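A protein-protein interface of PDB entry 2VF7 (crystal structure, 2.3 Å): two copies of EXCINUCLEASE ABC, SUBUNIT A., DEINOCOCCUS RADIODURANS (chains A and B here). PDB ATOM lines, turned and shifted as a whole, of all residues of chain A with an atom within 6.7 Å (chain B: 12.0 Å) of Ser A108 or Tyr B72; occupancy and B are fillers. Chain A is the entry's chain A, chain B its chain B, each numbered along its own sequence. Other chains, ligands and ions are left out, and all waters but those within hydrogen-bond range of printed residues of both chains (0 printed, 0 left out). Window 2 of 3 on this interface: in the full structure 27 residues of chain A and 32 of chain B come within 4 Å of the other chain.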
ATOM      1  N   GLN A  98       7.391   9.161 -13.622  1.00  0.00           N
ATOM      2  CA  GLN A  98       7.561   8.599 -12.280  1.00  0.00           C
ATOM      3  C   GLN A  98       6.350   8.894 -11.422  1.00  0.00           C
ATOM      4  O   GLN A  98       5.706   9.934 -11.572  1.00  0.00           O
ATOM      5  CB  GLN A  98       8.824   9.144 -11.611  1.00  0.00           C
ATOM      6  CG  GLN A  98       9.110   8.549 -10.224  1.00  0.00           C
ATOM      7  CD  GLN A  98      10.531   8.071 -10.080  1.00  0.00           C
ATOM      8  OE1 GLN A  98      11.329   8.706  -9.403  1.00  0.00           O
ATOM      9  NE2 GLN A  98      10.866   6.950 -10.733  1.00  0.00           N
ATOM     10  N   GLN A  99       6.047   7.977 -10.511  1.00  0.00           N
ATOM     11  CA  GLN A  99       4.959   8.151  -9.564  1.00  0.00           C
ATOM     12  C   GLN A  99       5.348   9.100  -8.419  1.00  0.00           C
ATOM     13  O   GLN A  99       6.531   9.261  -8.095  1.00  0.00           O
ATOM     14  CB  GLN A  99       4.577   6.783  -9.001  1.00  0.00           C
ATOM     15  CG  GLN A  99       3.093   6.538  -8.825  1.00  0.00           C
ATOM     16  CD  GLN A  99       2.832   5.135  -8.293  1.00  0.00           C
ATOM     17  OE1 GLN A  99       3.057   4.857  -7.108  1.00  0.00           O
ATOM     18  NE2 GLN A  99       2.372   4.233  -9.175  1.00  0.00           N
ATOM     19  N   PRO A 104       2.194   4.129  -2.961  1.00  0.00           N
ATOM     20  CA  PRO A 104       2.544   2.736  -3.246  1.00  0.00           C
ATOM     21  C   PRO A 104       2.500   2.465  -4.750  1.00  0.00           C
ATOM     22  O   PRO A 104       1.581   2.950  -5.425  1.00  0.00           O
ATOM     23  CB  PRO A 104       1.443   1.944  -2.533  1.00  0.00           C
ATOM     24  CG  PRO A 104       0.278   2.875  -2.473  1.00  0.00           C
ATOM     25  CD  PRO A 104       0.846   4.263  -2.376  1.00  0.00           C
ATOM     26  N   THR A 105       3.488   1.735  -5.277  1.00  0.00           N
ATOM     27  CA  THR A 105       3.420   1.285  -6.674  1.00  0.00           C
ATOM     28  C   THR A 105       2.323   0.216  -6.764  1.00  0.00           C
ATOM     29  O   THR A 105       2.207  -0.642  -5.883  1.00  0.00           O
ATOM     30  CB  THR A 105       4.778   0.747  -7.227  1.00  0.00           C
ATOM     31  OG1 THR A 105       5.779   1.773  -7.162  1.00  0.00           O
ATOM     32  CG2 THR A 105       4.651   0.317  -8.695  1.00  0.00           C
ATOM     33  N   ALA A 106       1.486   0.319  -7.800  1.00  0.00           N
ATOM     34  CA  ALA A 106       0.458  -0.678  -8.066  1.00  0.00           C
ATOM     35  C   ALA A 106       1.106  -1.917  -8.675  1.00  0.00           C
ATOM     36  O   ALA A 106       2.221  -1.848  -9.218  1.00  0.00           O
ATOM     37  CB  ALA A 106      -0.595  -0.112  -8.987  1.00  0.00           C
ATOM     38  N   ARG A 107       0.415  -3.048  -8.564  1.00  0.00           N
ATOM     39  CA  ARG A 107       0.905  -4.318  -9.086  1.00  0.00           C
ATOM     40  C   ARG A 107       0.631  -4.487 -10.577  1.00  0.00           C
ATOM     41  O   ARG A 107      -0.511  -4.395 -11.024  1.00  0.00           O
ATOM     42  CB  ARG A 107       0.299  -5.484  -8.305  1.00  0.00           C
ATOM     43  CG  ARG A 107       1.013  -5.796  -7.000  1.00  0.00           C
ATOM     44  CD  ARG A 107       2.350  -6.480  -7.261  1.00  0.00           C
ATOM     45  NE  ARG A 107       2.206  -7.879  -7.667  1.00  0.00           N
ATOM     46  CZ  ARG A 107       2.489  -8.925  -6.890  1.00  0.00           C
ATOM     47  NH1 ARG A 107       2.937  -8.741  -5.654  1.00  0.00           N
ATOM     48  NH2 ARG A 107       2.330 -10.161  -7.348  1.00  0.00           N
ATOM     49  N   SER A 108       1.702  -4.728 -11.327  1.00  0.00           N
ATOM     50  CA  SER A 108       1.657  -5.054 -12.751  1.00  0.00           C
ATOM     51  C   SER A 108       2.775  -6.028 -13.082  1.00  0.00           C
ATOM     52  O   SER A 108       3.499  -6.485 -12.199  1.00  0.00           O
ATOM     53  CB  SER A 108       1.836  -3.797 -13.617  1.00  0.00           C
ATOM     54  OG  SER A 108       0.655  -3.444 -14.320  1.00  0.00           O
ATOM     55  N   SER A 109       2.890  -6.329 -14.374  1.00  0.00           N
ATOM     56  CA  SER A 109       3.972  -7.116 -14.951  1.00  0.00           C
ATOM     57  C   SER A 109       4.677  -6.207 -15.932  1.00  0.00           C
ATOM     58  O   SER A 109       4.157  -5.151 -16.268  1.00  0.00           O
ATOM     59  CB  SER A 109       3.407  -8.299 -15.729  1.00  0.00           C
ATOM     60  OG  SER A 109       2.082  -8.579 -15.335  1.00  0.00           O
ATOM     61  N   VAL A 110       5.848  -6.615 -16.402  1.00  0.00           N
ATOM     62  CA  VAL A 110       6.546  -5.891 -17.460  1.00  0.00           C
ATOM     63  C   VAL A 110       5.723  -5.904 -18.767  1.00  0.00           C
ATOM     64  O   VAL A 110       5.602  -4.881 -19.454  1.00  0.00           O
ATOM     65  CB  VAL A 110       7.951  -6.485 -17.668  1.00  0.00           C
ATOM     66  CG1 VAL A 110       8.600  -5.981 -18.962  1.00  0.00           C
ATOM     67  CG2 VAL A 110       8.827  -6.187 -16.458  1.00  0.00           C
ATOM     68  N   GLY A 111       5.138  -7.059 -19.075  1.00  0.00           N
ATOM     69  CA  GLY A 111       4.287  -7.223 -20.240  1.00  0.00           C
ATOM     70  C   GLY A 111       2.971  -6.468 -20.237  1.00  0.00           C
ATOM     71  O   GLY A 111       2.321  -6.350 -21.279  1.00  0.00           O
ATOM     72  N   SER A 112       2.572  -5.959 -19.076  1.00  0.00           N
ATOM     73  CA  SER A 112       1.378  -5.121 -18.978  1.00  0.00           C
ATOM     74  C   SER A 112       1.706  -3.648 -19.162  1.00  0.00           C
ATOM     75  O   SER A 112       0.956  -2.917 -19.804  1.00  0.00           O
ATOM     76  CB  SER A 112       0.690  -5.311 -17.630  1.00  0.00           C
ATOM     77  OG  SER A 112       0.565  -6.680 -17.332  1.00  0.00           O
ATOM     78  N   VAL A 113       2.821  -3.213 -18.585  1.00  0.00           N
ATOM     79  CA  VAL A 113       3.229  -1.818 -18.667  1.00  0.00           C
ATOM     80  C   VAL A 113       3.766  -1.475 -20.050  1.00  0.00           C
ATOM     81  O   VAL A 113       3.775  -0.303 -20.449  1.00  0.00           O
ATOM     82  CB  VAL A 113       4.265  -1.445 -17.563  1.00  0.00           C
ATOM     83  CG1 VAL A 113       4.576   0.057 -17.579  1.00  0.00           C
ATOM     84  CG2 VAL A 113       3.737  -1.826 -16.190  1.00  0.00           C
ATOM     85  N   ASP A 374       6.753 -11.594 -17.302  1.00  0.00           N
ATOM     86  CA  ASP A 374       5.987 -11.954 -16.094  1.00  0.00           C
ATOM     87  C   ASP A 374       6.508 -11.256 -14.824  1.00  0.00           C
ATOM     88  O   ASP A 374       5.917 -11.370 -13.747  1.00  0.00           O
ATOM     89  CB  ASP A 374       5.914 -13.484 -15.914  1.00  0.00           C
ATOM     90  CG  ASP A 374       7.294 -14.145 -15.736  1.00  0.00           C
ATOM     91  OD1 ASP A 374       8.339 -13.459 -15.826  1.00  0.00           O
ATOM     92  OD2 ASP A 374       7.329 -15.378 -15.500  1.00  0.00           O
ATOM     93  N   ARG A 375       7.605 -10.517 -14.975  1.00  0.00           N
ATOM     94  CA  ARG A 375       8.283  -9.837 -13.878  1.00  0.00           C
ATOM     95  C   ARG A 375       7.427  -8.727 -13.284  1.00  0.00           C
ATOM     96  O   ARG A 375       6.941  -7.836 -14.004  1.00  0.00           O
ATOM     97  CB  ARG A 375       9.622  -9.284 -14.384  1.00  0.00           C
ATOM     98  CG  ARG A 375      10.368  -8.365 -13.443  1.00  0.00           C
ATOM     99  CD  ARG A 375      11.160  -9.135 -12.422  1.00  0.00           C
ATOM    100  NE  ARG A 375      11.940  -8.248 -11.569  1.00  0.00           N
ATOM    101  CZ  ARG A 375      13.219  -7.941 -11.768  1.00  0.00           C
ATOM    102  NH1 ARG A 375      13.884  -8.450 -12.797  1.00  0.00           N
ATOM    103  NH2 ARG A 375      13.836  -7.117 -10.933  1.00  0.00           N
ATOM    104  N   SER A 376       7.260  -8.797 -11.963  1.00  0.00           N
ATOM    105  CA  SER A 376       6.430  -7.884 -11.180  1.00  0.00           C
ATOM    106  C   SER A 376       7.052  -6.509 -11.058  1.00  0.00           C
ATOM    107  O   SER A 376       8.248  -6.388 -10.814  1.00  0.00           O
ATOM    108  CB  SER A 376       6.211  -8.451  -9.775  1.00  0.00           C
ATOM    109  OG  SER A 376       4.867  -8.851  -9.585  1.00  0.00           O
ATOM    110  N   THR A 377       6.226  -5.477 -11.199  1.00  0.00           N
ATOM    111  CA  THR A 377       6.703  -4.099 -11.189  1.00  0.00           C
ATOM    112  C   THR A 377       7.289  -3.578  -9.867  1.00  0.00           C
ATOM    113  O   THR A 377       8.151  -2.693  -9.896  1.00  0.00           O
ATOM    114  CB  THR A 377       5.638  -3.098 -11.717  1.00  0.00           C
ATOM    115  OG1 THR A 377       4.356  -3.439 -11.190  1.00  0.00           O
ATOM    116  CG2 THR A 377       5.579  -3.143 -13.239  1.00  0.00           C
ATOM    117  N   PRO A 378       6.808  -4.077  -8.713  1.00  0.00           N
ATOM    118  CA  PRO A 378       7.439  -3.637  -7.473  1.00  0.00           C
ATOM    119  C   PRO A 378       8.798  -4.305  -7.185  1.00  0.00           C
ATOM    120  O   PRO A 378       9.508  -3.888  -6.260  1.00  0.00           O
ATOM    121  CB  PRO A 378       6.408  -4.025  -6.397  1.00  0.00           C
ATOM    122  CG  PRO A 378       5.186  -4.462  -7.141  1.00  0.00           C
ATOM    123  CD  PRO A 378       5.675  -4.973  -8.435  1.00  0.00           C
ATOM    124  N   LEU A 385      11.830   0.810 -14.036  1.00  0.00           N
ATOM    125  CA  LEU A 385      10.456   1.079 -14.482  1.00  0.00           C
ATOM    126  C   LEU A 385      10.236   2.416 -15.149  1.00  0.00           C
ATOM    127  O   LEU A 385       9.290   2.567 -15.906  1.00  0.00           O
ATOM    128  CB  LEU A 385       9.385   0.820 -13.414  1.00  0.00           C
ATOM    129  CG  LEU A 385       9.432   1.250 -11.958  1.00  0.00           C
ATOM    130  CD1 LEU A 385       9.572   2.756 -11.772  1.00  0.00           C
ATOM    131  CD2 LEU A 385       8.147   0.786 -11.314  1.00  0.00           C
ATOM    132  N   ARG A 389       8.931   2.843 -19.034  1.00  0.00           N
ATOM    133  CA  ARG A 389       7.814   3.749 -19.259  1.00  0.00           C
ATOM    134  C   ARG A 389       8.162   4.725 -20.373  1.00  0.00           C
ATOM    135  O   ARG A 389       7.306   5.134 -21.156  1.00  0.00           O
ATOM    136  CB  ARG A 389       7.440   4.456 -17.975  1.00  0.00           C
ATOM    137  CG  ARG A 389       5.967   4.730 -17.910  1.00  0.00           C
ATOM    138  CD  ARG A 389       5.322   4.221 -16.632  1.00  0.00           C
ATOM    139  NE  ARG A 389       4.972   5.297 -15.701  1.00  0.00           N
ATOM    140  CZ  ARG A 389       4.042   6.239 -15.904  1.00  0.00           C
ATOM    141  NH1 ARG A 389       3.345   6.294 -17.040  1.00  0.00           N
ATOM    142  NH2 ARG A 389       3.817   7.147 -14.962  1.00  0.00           N
ATOM    143  N   PRO A 658      -3.567   7.733  -8.054  1.00  0.00           N
ATOM    144  CA  PRO A 658      -2.967   7.615  -6.729  1.00  0.00           C
ATOM    145  C   PRO A 658      -3.325   8.750  -5.773  1.00  0.00           C
ATOM    146  O   PRO A 658      -3.038   9.919  -6.049  1.00  0.00           O
ATOM    147  CB  PRO A 658      -1.471   7.584  -7.047  1.00  0.00           C
ATOM    148  CG  PRO A 658      -1.404   6.851  -8.395  1.00  0.00           C
ATOM    149  CD  PRO A 658      -2.806   6.931  -9.031  1.00  0.00           C
ATOM    150  N   ARG B  63      -8.097   8.261 -24.785  1.00  0.00           N
ATOM    151  CA  ARG B  63      -7.585   6.949 -24.411  1.00  0.00           C
ATOM    152  C   ARG B  63      -6.073   6.974 -24.198  1.00  0.00           C
ATOM    153  O   ARG B  63      -5.580   6.408 -23.227  1.00  0.00           O
ATOM    154  CB  ARG B  63      -7.932   5.893 -25.464  1.00  0.00           C
ATOM    155  CG  ARG B  63      -8.152   4.511 -24.886  1.00  0.00           C
ATOM    156  CD  ARG B  63      -7.884   3.422 -25.898  1.00  0.00           C
ATOM    157  NE  ARG B  63      -6.451   3.280 -26.159  1.00  0.00           N
ATOM    158  CZ  ARG B  63      -5.840   3.677 -27.274  1.00  0.00           C
ATOM    159  NH1 ARG B  63      -6.542   4.235 -28.250  1.00  0.00           N
ATOM    160  NH2 ARG B  63      -4.530   3.511 -27.416  1.00  0.00           N
ATOM    161  N   ARG B  64      -5.356   7.634 -25.108  1.00  0.00           N
ATOM    162  CA  ARG B  64      -3.890   7.644 -25.135  1.00  0.00           C
ATOM    163  C   ARG B  64      -3.248   8.448 -24.016  1.00  0.00           C
ATOM    164  O   ARG B  64      -2.093   8.219 -23.663  1.00  0.00           O
ATOM    165  CB  ARG B  64      -3.396   8.233 -26.442  1.00  0.00           C
ATOM    166  CG  ARG B  64      -3.590   7.388 -27.650  1.00  0.00           C
ATOM    167  CD  ARG B  64      -3.200   8.235 -28.806  1.00  0.00           C
ATOM    168  NE  ARG B  64      -2.935   7.465 -30.007  1.00  0.00           N
ATOM    169  CZ  ARG B  64      -2.791   8.015 -31.207  1.00  0.00           C
ATOM    170  NH1 ARG B  64      -2.892   9.335 -31.354  1.00  0.00           N
ATOM    171  NH2 ARG B  64      -2.549   7.248 -32.262  1.00  0.00           N
ATOM    172  N   TYR B  65      -3.980   9.423 -23.500  1.00  0.00           N
ATOM    173  CA  TYR B  65      -3.497  10.241 -22.424  1.00  0.00           C
ATOM    174  C   TYR B  65      -3.733   9.510 -21.113  1.00  0.00           C
ATOM    175  O   TYR B  65      -2.800   9.348 -20.320  1.00  0.00           O
ATOM    176  CB  TYR B  65      -4.203  11.590 -22.439  1.00  0.00           C
ATOM    177  CG  TYR B  65      -3.814  12.529 -21.320  1.00  0.00           C
ATOM    178  CD1 TYR B  65      -2.646  13.281 -21.395  1.00  0.00           C
ATOM    179  CD2 TYR B  65      -4.616  12.668 -20.184  1.00  0.00           C
ATOM    180  CE1 TYR B  65      -2.277  14.148 -20.371  1.00  0.00           C
ATOM    181  CE2 TYR B  65      -4.253  13.537 -19.139  1.00  0.00           C
ATOM    182  CZ  TYR B  65      -3.088  14.274 -19.249  1.00  0.00           C
ATOM    183  OH  TYR B  65      -2.726  15.147 -18.248  1.00  0.00           O
ATOM    184  N   LEU B  66      -4.973   9.063 -20.897  1.00  0.00           N
ATOM    185  CA  LEU B  66      -5.359   8.357 -19.669  1.00  0.00           C
ATOM    186  C   LEU B  66      -4.529   7.096 -19.396  1.00  0.00           C
ATOM    187  O   LEU B  66      -4.247   6.783 -18.239  1.00  0.00           O
ATOM    188  CB  LEU B  66      -6.853   8.002 -19.676  1.00  0.00           C
ATOM    189  CG  LEU B  66      -7.919   9.069 -19.953  1.00  0.00           C
ATOM    190  CD1 LEU B  66      -9.317   8.472 -19.737  1.00  0.00           C
ATOM    191  CD2 LEU B  66      -7.733  10.342 -19.122  1.00  0.00           C
ATOM    192  N   GLU B  67      -4.149   6.387 -20.462  1.00  0.00           N
ATOM    193  CA  GLU B  67      -3.265   5.221 -20.378  1.00  0.00           C
ATOM    194  C   GLU B  67      -1.838   5.600 -20.034  1.00  0.00           C
ATOM    195  O   GLU B  67      -1.072   4.767 -19.563  1.00  0.00           O
ATOM    196  CB  GLU B  67      -3.232   4.476 -21.706  1.00  0.00           C
ATOM    197  CG  GLU B  67      -4.456   3.660 -22.013  1.00  0.00           C
ATOM    198  CD  GLU B  67      -4.268   2.780 -23.235  1.00  0.00           C
ATOM    199  OE1 GLU B  67      -3.108   2.414 -23.537  1.00  0.00           O
ATOM    200  OE2 GLU B  67      -5.279   2.449 -23.895  1.00  0.00           O
ATOM    201  N   SER B  68      -1.468   6.846 -20.317  1.00  0.00           N
ATOM    202  CA  SER B  68      -0.087   7.301 -20.140  1.00  0.00           C
ATOM    203  C   SER B  68       0.095   7.915 -18.764  1.00  0.00           C
ATOM    204  O   SER B  68       1.174   7.826 -18.173  1.00  0.00           O
ATOM    205  CB  SER B  68       0.295   8.307 -21.228  1.00  0.00           C
ATOM    206  OG  SER B  68       0.150   7.726 -22.515  1.00  0.00           O
ATOM    207  N   VAL B  69      -0.976   8.539 -18.273  1.00  0.00           N
ATOM    208  CA  VAL B  69      -1.008   9.138 -16.948  1.00  0.00           C
ATOM    209  C   VAL B  69      -1.129   8.071 -15.863  1.00  0.00           C
ATOM    210  O   VAL B  69      -0.402   8.130 -14.873  1.00  0.00           O
ATOM    211  CB  VAL B  69      -2.128  10.184 -16.829  1.00  0.00           C
ATOM    212  CG1 VAL B  69      -2.594  10.316 -15.386  1.00  0.00           C
ATOM    213  CG2 VAL B  69      -1.650  11.525 -17.381  1.00  0.00           C
ATOM    214  N   SER B  70      -2.018   7.097 -16.061  1.00  0.00           N
ATOM    215  CA  SER B  70      -2.150   5.951 -15.158  1.00  0.00           C
ATOM    216  C   SER B  70      -2.125   4.647 -15.954  1.00  0.00           C
ATOM    217  O   SER B  70      -3.168   4.196 -16.421  1.00  0.00           O
ATOM    218  CB  SER B  70      -3.440   6.048 -14.333  1.00  0.00           C
ATOM    219  OG  SER B  70      -3.292   6.944 -13.236  1.00  0.00           O
ATOM    220  N   PRO B  71      -0.930   4.043 -16.126  1.00  0.00           N
ATOM    221  CA  PRO B  71      -0.772   2.837 -16.956  1.00  0.00           C
ATOM    222  C   PRO B  71      -1.568   1.629 -16.449  1.00  0.00           C
ATOM    223  O   PRO B  71      -2.637   1.322 -16.991  1.00  0.00           O
ATOM    224  CB  PRO B  71       0.738   2.559 -16.891  1.00  0.00           C
ATOM    225  CG  PRO B  71       1.345   3.844 -16.488  1.00  0.00           C
ATOM    226  CD  PRO B  71       0.361   4.472 -15.559  1.00  0.00           C
ATOM    227  N   TYR B  72      -1.024   0.964 -15.427  1.00  0.00           N
ATOM    228  CA  TYR B  72      -1.647  -0.163 -14.713  1.00  0.00           C
ATOM    229  C   TYR B  72      -3.179  -0.107 -14.573  1.00  0.00           C
ATOM    230  O   TYR B  72      -3.906  -0.629 -15.433  1.00  0.00           O
ATOM    231  CB  TYR B  72      -0.999  -0.302 -13.327  1.00  0.00           C
ATOM    232  CG  TYR B  72      -0.159   0.901 -12.934  1.00  0.00           C
ATOM    233  CD1 TYR B  72      -0.887   2.302 -12.784  1.00  0.00           C
ATOM    234  CD2 TYR B  72       1.303   0.660 -12.767  1.00  0.00           C
ATOM    235  CE1 TYR B  72      -0.131   3.407 -12.492  1.00  0.00           C
ATOM    236  CE2 TYR B  72       2.065   1.757 -12.439  1.00  0.00           C
ATOM    237  CZ  TYR B  72       1.444   3.122 -12.238  1.00  0.00           C
ATOM    238  OH  TYR B  72       2.225   4.207 -11.893  1.00  0.00           O
ATOM    239  N   ALA B  73      -3.649   0.531 -13.497  1.00  0.00           N
ATOM    240  CA  ALA B  73      -5.074   0.578 -13.134  1.00  0.00           C
ATOM    241  C   ALA B  73      -5.995   1.116 -14.233  1.00  0.00           C
ATOM    242  O   ALA B  73      -7.122   0.639 -14.384  1.00  0.00           O
ATOM    243  CB  ALA B  73      -5.267   1.368 -11.848  1.00  0.00           C
ATOM    244  N   ARG B  74      -5.523   2.111 -14.983  1.00  0.00           N
ATOM    245  CA  ARG B  74      -6.292   2.675 -16.098  1.00  0.00           C
ATOM    246  C   ARG B  74      -5.702   2.286 -17.470  1.00  0.00           C
ATOM    247  O   ARG B  74      -5.227   3.128 -18.240  1.00  0.00           O
ATOM    248  CB  ARG B  74      -6.507   4.198 -15.922  1.00  0.00           C
ATOM    249  CG  ARG B  74      -6.865   5.010 -17.187  1.00  0.00           C
ATOM    250  CD  ARG B  74      -8.177   4.594 -17.843  1.00  0.00           C
ATOM    251  NE  ARG B  74      -8.103   4.706 -19.300  1.00  0.00           N
ATOM    252  CZ  ARG B  74      -8.117   3.676 -20.145  1.00  0.00           C
ATOM    253  NH1 ARG B  74      -8.228   2.431 -19.696  1.00  0.00           N
ATOM    254  NH2 ARG B  74      -8.043   3.888 -21.450  1.00  0.00           N
ATOM    255  N   ARG B  75      -5.704   0.985 -17.733  1.00  0.00           N
ATOM    256  CA  ARG B  75      -5.618   0.468 -19.088  1.00  0.00           C
ATOM    257  C   ARG B  75      -6.780  -0.507 -19.153  1.00  0.00           C
ATOM    258  O   ARG B  75      -6.822  -1.408 -19.997  1.00  0.00           O
ATOM    259  CB  ARG B  75      -4.280  -0.237 -19.334  1.00  0.00           C
ATOM    260  CG  ARG B  75      -3.767  -0.124 -20.777  1.00  0.00           C
ATOM    261  CD  ARG B  75      -2.548  -1.014 -21.042  1.00  0.00           C
ATOM    262  NE  ARG B  75      -1.422  -0.734 -20.147  1.00  0.00           N
ATOM    263  CZ  ARG B  75      -0.421   0.106 -20.412  1.00  0.00           C
ATOM    264  NH1 ARG B  75      -0.376   0.777 -21.556  1.00  0.00           N
ATOM    265  NH2 ARG B  75       0.546   0.281 -19.521  1.00  0.00           N
ATOM    266  N   LEU B  76      -7.733  -0.296 -18.241  1.00  0.00           N
ATOM    267  CA  LEU B  76      -8.820  -1.238 -17.979  1.00  0.00           C
ATOM    268  C   LEU B  76     -10.218  -0.628 -18.127  1.00  0.00           C
ATOM    269  O   LEU B  76     -11.180  -1.354 -18.367  1.00  0.00           O
ATOM    270  CB  LEU B  76      -8.659  -1.871 -16.587  1.00  0.00           C
ATOM    271  CG  LEU B  76      -7.373  -2.634 -16.244  1.00  0.00           C
ATOM    272  CD1 LEU B  76      -7.518  -3.343 -14.896  1.00  0.00           C
ATOM    273  CD2 LEU B  76      -6.983  -3.629 -17.342  1.00  0.00           C
ATOM    274  N   PHE B  77     -10.325   0.694 -17.979  1.00  0.00           N
ATOM    275  CA  PHE B  77     -11.588   1.424 -18.193  1.00  0.00           C
ATOM    276  C   PHE B  77     -12.170   1.119 -19.572  1.00  0.00           C
ATOM    277  O   PHE B  77     -13.391   1.032 -19.745  1.00  0.00           O
ATOM    278  CB  PHE B  77     -11.362   2.934 -18.013  1.00  0.00           C
ATOM    279  CG  PHE B  77     -12.076   3.802 -19.030  1.00  0.00           C
ATOM    280  CD1 PHE B  77     -11.458   4.146 -20.241  1.00  0.00           C
ATOM    281  CD2 PHE B  77     -13.354   4.296 -18.769  1.00  0.00           C
ATOM    282  CE1 PHE B  77     -12.110   4.953 -21.178  1.00  0.00           C
ATOM    283  CE2 PHE B  77     -14.013   5.105 -19.702  1.00  0.00           C
ATOM    284  CZ  PHE B  77     -13.390   5.432 -20.907  1.00  0.00           C
ATOM    285  N   ASN B  78     -11.261   0.960 -20.532  1.00  0.00           N
ATOM    286  CA  ASN B  78     -11.552   0.595 -21.911  1.00  0.00           C
ATOM    287  C   ASN B  78     -12.249  -0.772 -22.079  1.00  0.00           C
ATOM    288  O   ASN B  78     -12.040  -1.466 -23.080  1.00  0.00           O
ATOM    289  CB  ASN B  78     -10.240   0.635 -22.706  1.00  0.00           C
ATOM    290  CG  ASN B  78      -9.084  -0.071 -21.981  1.00  0.00           C
ATOM    291  OD1 ASN B  78      -9.306  -0.943 -21.134  1.00  0.00           O
ATOM    292  ND2 ASN B  78      -7.849   0.305 -22.318  1.00  0.00           N
ATOM    293  N   GLN B  79     -13.074  -1.137 -21.094  1.00  0.00           N
ATOM    294  CA  GLN B  79     -13.880  -2.366 -21.105  1.00  0.00           C
ATOM    295  C   GLN B  79     -15.054  -2.299 -22.087  1.00  0.00           C
ATOM    296  O   GLN B  79     -15.715  -3.310 -22.358  1.00  0.00           O
ATOM    297  CB  GLN B  79     -14.412  -2.661 -19.698  1.00  0.00           C
ATOM    298  CG  GLN B  79     -13.450  -3.417 -18.791  1.00  0.00           C
ATOM    299  CD  GLN B  79     -13.846  -3.352 -17.321  1.00  0.00           C
ATOM    300  OE1 GLN B  79     -13.037  -2.984 -16.469  1.00  0.00           O
ATOM    301  NE2 GLN B  79     -15.093  -3.705 -17.020  1.00  0.00           N
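Of the 17 printed residues of chain B, 4 touch a printed residue of chain A. Hydrophobic or aromatic side chains of chain B that line the printed part of chain A: Pro B71 and Tyr B72. Of the 20 printed residues of chain A, 5 touch a printed residue of chain B. Along chain A the printed residues that touch a printed residue of chain B span positions 99 to 389.
Of chain B, only Tyr B72 (2.7 Å) comes within 4 Å of Gln A99. Arg A107 touches none of the printed residues of chain B. Of the printed residues of chain B, Ser A108 touches Tyr B72 (3.7 Å). No residue of chain B comes within 4 Å of Ser A109. No residue of chain B comes within 4 Å of Gly A111. Ser A112 touches just one residue of chain B: Arg B75. Printed residues of chain B within 4 Å of Val A113: Arg B75 (3.4 Å). No residue of chain B comes within 4 Å of Thr A377. Printed residues of chain A within 4 Å of Pro B71: Arg A389. Tyr B72 touches just these residues of chain A: Gln A99 (2.7 Å) and Ser A108 (3.7 Å). Of the printed residues of chain A, Arg B75 touches Ser A112 (3.2 Å) and Val A113 (3.4 Å). The nearest printed residue of chain B that does not touch Ser A108 is Ala B73 (5.9 Å).
The backbone carbonyl oxygen (O) of Pro A104 sits close to the side-chain amide oxygen (OE1) of Gln A99, at 2.9 Å. N of Ser A108 sits at hydrogen-bond distance from OG1 of Thr A377 (3.0 Å). The side-chain hydroxyl (OG) of Ser A109 is in hydrogen-bond range of the side-chain hydroxyl (OG) of Ser A112 (3.1 Å). O of Arg B64 sits at hydrogen-bond distance from OG of Ser B68, 2.6 Å away. The side-chain carboxylate (OE1) of Glu B67 is in salt-bridge range of the guanidinium group (NH1) of Arg B75 (3.8 Å). O of Arg B75 lies close to OD1 of Asn B78, 2.8 Å away.
The side-chain amide nitrogen (NE2) of Gln A99 lies within hydrogen-bond range of the side-chain hydroxyl (OH) of Tyr B72 (2.7 Å). The backbone carbonyl oxygen (O) of Ser A112 sits at hydrogen-bond distance from the guanidinium group (NH2) of Arg B75, 3.2 Å away. The backbone carbonyl oxygen (O) of Val A113 is in hydrogen-bond range of the guanidinium group (NH2) of Arg B75 (3.4 Å). NH1 of Arg A389 is in hydrogen-bond range of O of Ser B68 (2.9 Å).
Tyr B72 touches Ser A108 (CB to OG, 3.7 Å). Arg A389 touches Pro B71.
No position is printed for both chains.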
